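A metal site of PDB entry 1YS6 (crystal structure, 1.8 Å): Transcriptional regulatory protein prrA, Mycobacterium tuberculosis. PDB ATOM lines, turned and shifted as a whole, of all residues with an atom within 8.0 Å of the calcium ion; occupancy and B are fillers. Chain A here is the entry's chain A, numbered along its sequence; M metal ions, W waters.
The backbone carbonyl oxygen (O) of Val 13 lies within hydrogen-bond range of the backbone NH (N) of Asp 58. NZ of Lys 108 is in salt-bridge range of OD1 of Asp 58, at 2.9 Å.
The nearest printed residue that does not touch the calcium ion is Asp 14 (4.2 Å).
The calcium ion is bound by water W1 (2.2 Å), the side-chain carboxylate (OD1) of Asp 15 (2.2 Å), the side-chain carboxylate (OD2) of Asp 58 (2.3 Å), the backbone carbonyl oxygen (O) of Asn 60 (2.3 Å), water W2 (2.4 Å) and water W3 (2.5 Å).
Water W2 bridges the side-chain carboxylate (OD1) of Asp 14 and the side-chain amino group (NZ) of Lys 108.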
ATOM      1  N   VAL A  13     -29.948  -6.957  20.383  1.00  0.00           N
ATOM      2  CA  VAL A  13     -28.664  -6.564  19.817  1.00  0.00           C
ATOM      3  C   VAL A  13     -27.853  -7.799  19.414  1.00  0.00           C
ATOM      4  O   VAL A  13     -27.483  -8.621  20.256  1.00  0.00           O
ATOM      5  CB  VAL A  13     -27.824  -5.790  20.827  1.00  0.00           C
ATOM      6  CG1 VAL A  13     -26.587  -5.186  20.129  1.00  0.00           C
ATOM      7  CG2 VAL A  13     -28.659  -4.720  21.510  1.00  0.00           C
ATOM      8  N   ASP A  14     -27.596  -7.913  18.122  1.00  0.00           N
ATOM      9  CA  ASP A  14     -26.870  -9.067  17.577  1.00  0.00           C
ATOM     10  C   ASP A  14     -26.297  -8.677  16.240  1.00  0.00           C
ATOM     11  O   ASP A  14     -27.002  -8.072  15.431  1.00  0.00           O
ATOM     12  CB  ASP A  14     -27.787 -10.296  17.504  1.00  0.00           C
ATOM     13  CG  ASP A  14     -27.004 -11.607  17.522  1.00  0.00           C
ATOM     14  OD1 ASP A  14     -26.207 -11.810  16.600  1.00  0.00           O
ATOM     15  OD2 ASP A  14     -27.158 -12.386  18.502  1.00  0.00           O
ATOM     16  N   ASP A  15     -25.015  -9.015  16.002  1.00  0.00           N
ATOM     17  CA  ASP A  15     -24.338  -8.583  14.808  1.00  0.00           C
ATOM     18  C   ASP A  15     -24.585  -9.616  13.690  1.00  0.00           C
ATOM     19  O   ASP A  15     -24.244  -9.392  12.527  1.00  0.00           O
ATOM     20  CB  ASP A  15     -22.810  -8.428  15.045  1.00  0.00           C
ATOM     21  CG  ASP A  15     -22.134  -9.775  15.344  1.00  0.00           C
ATOM     22  OD1 ASP A  15     -22.595 -10.505  16.246  1.00  0.00           O
ATOM     23  OD2 ASP A  15     -21.128 -10.082  14.727  1.00  0.00           O
ATOM     24  N   ASP A  16     -25.193 -10.732  14.046  1.00  0.00           N
ATOM     25  CA  ASP A  16     -25.547 -11.691  13.022  1.00  0.00           C
ATOM     26  C   ASP A  16     -26.954 -11.370  12.509  1.00  0.00           C
ATOM     27  O   ASP A  16     -27.927 -11.562  13.227  1.00  0.00           O
ATOM     28  CB  ASP A  16     -25.488 -13.090  13.617  1.00  0.00           C
ATOM     29  CG  ASP A  16     -25.875 -14.153  12.620  1.00  0.00           C
ATOM     30  OD1 ASP A  16     -25.282 -15.249  12.682  1.00  0.00           O
ATOM     31  OD2 ASP A  16     -26.751 -13.883  11.783  1.00  0.00           O
ATOM     32  N   VAL A  19     -29.846 -14.106  12.986  1.00  0.00           N
ATOM     33  CA  VAL A  19     -30.255 -14.242  14.373  1.00  0.00           C
ATOM     34  C   VAL A  19     -31.047 -13.000  14.784  1.00  0.00           C
ATOM     35  O   VAL A  19     -32.084 -13.100  15.435  1.00  0.00           O
ATOM     36  CB  VAL A  19     -28.996 -14.426  15.263  1.00  0.00           C
ATOM     37  CG1 VAL A  19     -29.337 -14.420  16.729  1.00  0.00           C
ATOM     38  CG2 VAL A  19     -28.316 -15.742  14.903  1.00  0.00           C
ATOM     39  N   VAL A  38     -27.313  -3.561  15.504  1.00  0.00           N
ATOM     40  CA  VAL A  38     -26.418  -4.507  14.860  1.00  0.00           C
ATOM     41  C   VAL A  38     -25.064  -4.653  15.536  1.00  0.00           C
ATOM     42  O   VAL A  38     -24.273  -5.555  15.211  1.00  0.00           O
ATOM     43  CB  VAL A  38     -26.222  -4.097  13.378  1.00  0.00           C
ATOM     44  CG1 VAL A  38     -27.559  -4.145  12.594  1.00  0.00           C
ATOM     45  CG2 VAL A  38     -25.573  -2.699  13.303  1.00  0.00           C
ATOM     46  N   ASP A  58     -26.177  -9.612  22.653  1.00  0.00           N
ATOM     47  CA  ASP A  58     -25.121 -10.577  22.222  1.00  0.00           C
ATOM     48  C   ASP A  58     -23.780 -10.091  22.765  1.00  0.00           C
ATOM     49  O   ASP A  58     -23.561  -8.874  22.826  1.00  0.00           O
ATOM     50  CB  ASP A  58     -25.096 -10.573  20.722  1.00  0.00           C
ATOM     51  CG  ASP A  58     -24.180 -11.626  20.160  1.00  0.00           C
ATOM     52  OD1 ASP A  58     -24.165 -12.735  20.678  1.00  0.00           O
ATOM     53  OD2 ASP A  58     -23.511 -11.302  19.189  1.00  0.00           O
ATOM     54  N   ILE A  59     -22.818 -10.977  22.954  1.00  0.00           N
ATOM     55  CA  ILE A  59     -21.555 -10.570  23.576  1.00  0.00           C
ATOM     56  C   ILE A  59     -20.545 -10.248  22.487  1.00  0.00           C
ATOM     57  O   ILE A  59     -20.041  -9.110  22.421  1.00  0.00           O
ATOM     58  CB  ILE A  59     -21.009 -11.643  24.561  1.00  0.00           C
ATOM     59  CG1 ILE A  59     -21.811 -11.661  25.863  1.00  0.00           C
ATOM     60  CG2 ILE A  59     -19.512 -11.361  24.883  1.00  0.00           C
ATOM     61  CD1 ILE A  59     -22.178 -10.283  26.435  1.00  0.00           C
ATOM     62  N   ASN A  60     -20.287 -11.218  21.616  1.00  0.00           N
ATOM     63  CA  ASN A  60     -19.278 -11.026  20.583  1.00  0.00           C
ATOM     64  C   ASN A  60     -19.805 -10.292  19.340  1.00  0.00           C
ATOM     65  O   ASN A  60     -20.500 -10.867  18.496  1.00  0.00           O
ATOM     66  CB  ASN A  60     -18.548 -12.352  20.256  1.00  0.00           C
ATOM     67  CG  ASN A  60     -17.758 -12.904  21.461  1.00  0.00           C
ATOM     68  OD1 ASN A  60     -17.055 -12.171  22.155  1.00  0.00           O
ATOM     69  ND2 ASN A  60     -17.884 -14.193  21.699  1.00  0.00           N
ATOM     70  N   MET A  61     -19.420  -9.013  19.242  1.00  0.00           N
ATOM     71  CA  MET A  61     -19.872  -8.121  18.148  1.00  0.00           C
ATOM     72  C   MET A  61     -18.704  -7.232  17.752  1.00  0.00           C
ATOM     73  O   MET A  61     -17.877  -6.905  18.632  1.00  0.00           O
ATOM     74  CB  MET A  61     -21.047  -7.230  18.605  1.00  0.00           C
ATOM     75  CG  MET A  61     -22.314  -7.956  19.039  1.00  0.00           C
ATOM     76  SD  MET A  61     -23.589  -6.819  19.420  1.00  0.00           S
ATOM     77  CE  MET A  61     -22.791  -6.119  20.834  1.00  0.00           C
ATOM     78  N   PRO A  62     -18.672  -6.758  16.473  1.00  0.00           N
ATOM     79  CA  PRO A  62     -17.689  -5.777  16.086  1.00  0.00           C
ATOM     80  C   PRO A  62     -18.053  -4.392  16.595  1.00  0.00           C
ATOM     81  O   PRO A  62     -19.128  -4.231  17.150  1.00  0.00           O
ATOM     82  CB  PRO A  62     -17.742  -5.809  14.558  1.00  0.00           C
ATOM     83  CG  PRO A  62     -19.168  -6.168  14.260  1.00  0.00           C
ATOM     84  CD  PRO A  62     -19.576  -7.088  15.347  1.00  0.00           C
ATOM     85  N   LEU A  85     -26.423 -12.751  25.673  1.00  0.00           N
ATOM     86  CA  LEU A  85     -26.412 -14.034  24.968  1.00  0.00           C
ATOM     87  C   LEU A  85     -24.922 -14.362  24.832  1.00  0.00           C
ATOM     88  O   LEU A  85     -24.196 -13.641  24.093  1.00  0.00           O
ATOM     89  CB  LEU A  85     -27.067 -13.922  23.589  1.00  0.00           C
ATOM     90  CG  LEU A  85     -28.462 -13.285  23.478  1.00  0.00           C
ATOM     91  CD1 LEU A  85     -28.971 -13.261  22.008  1.00  0.00           C
ATOM     92  CD2 LEU A  85     -29.458 -14.022  24.397  1.00  0.00           C
ATOM     93  N   LYS A 108     -26.382 -19.492  23.602  1.00  0.00           N
ATOM     94  CA  LYS A 108     -26.773 -19.896  22.265  1.00  0.00           C
ATOM     95  C   LYS A 108     -26.187 -21.288  22.026  1.00  0.00           C
ATOM     96  O   LYS A 108     -25.045 -21.537  22.398  1.00  0.00           O
ATOM     97  CB  LYS A 108     -26.157 -18.980  21.216  1.00  0.00           C
ATOM     98  CG  LYS A 108     -26.560 -17.501  21.296  1.00  0.00           C
ATOM     99  CD  LYS A 108     -25.608 -16.649  20.464  1.00  0.00           C
ATOM    100  CE  LYS A 108     -26.366 -15.462  19.825  1.00  0.00           C
ATOM    101  NZ  LYS A 108     -25.547 -14.580  18.963  1.00  0.00           N
HETATM  102 CA    CA M   1     -22.147 -12.178  17.625  1.00  0.00          CA
HETATM  103  O   HOH W   1     -21.776 -13.676  19.202  1.00  0.00           O
HETATM  104  O   HOH W   2     -24.122 -13.378  16.901  1.00  0.00           O
HETATM  105  O   HOH W   3     -20.371 -12.309  15.817  1.00  0.00           O
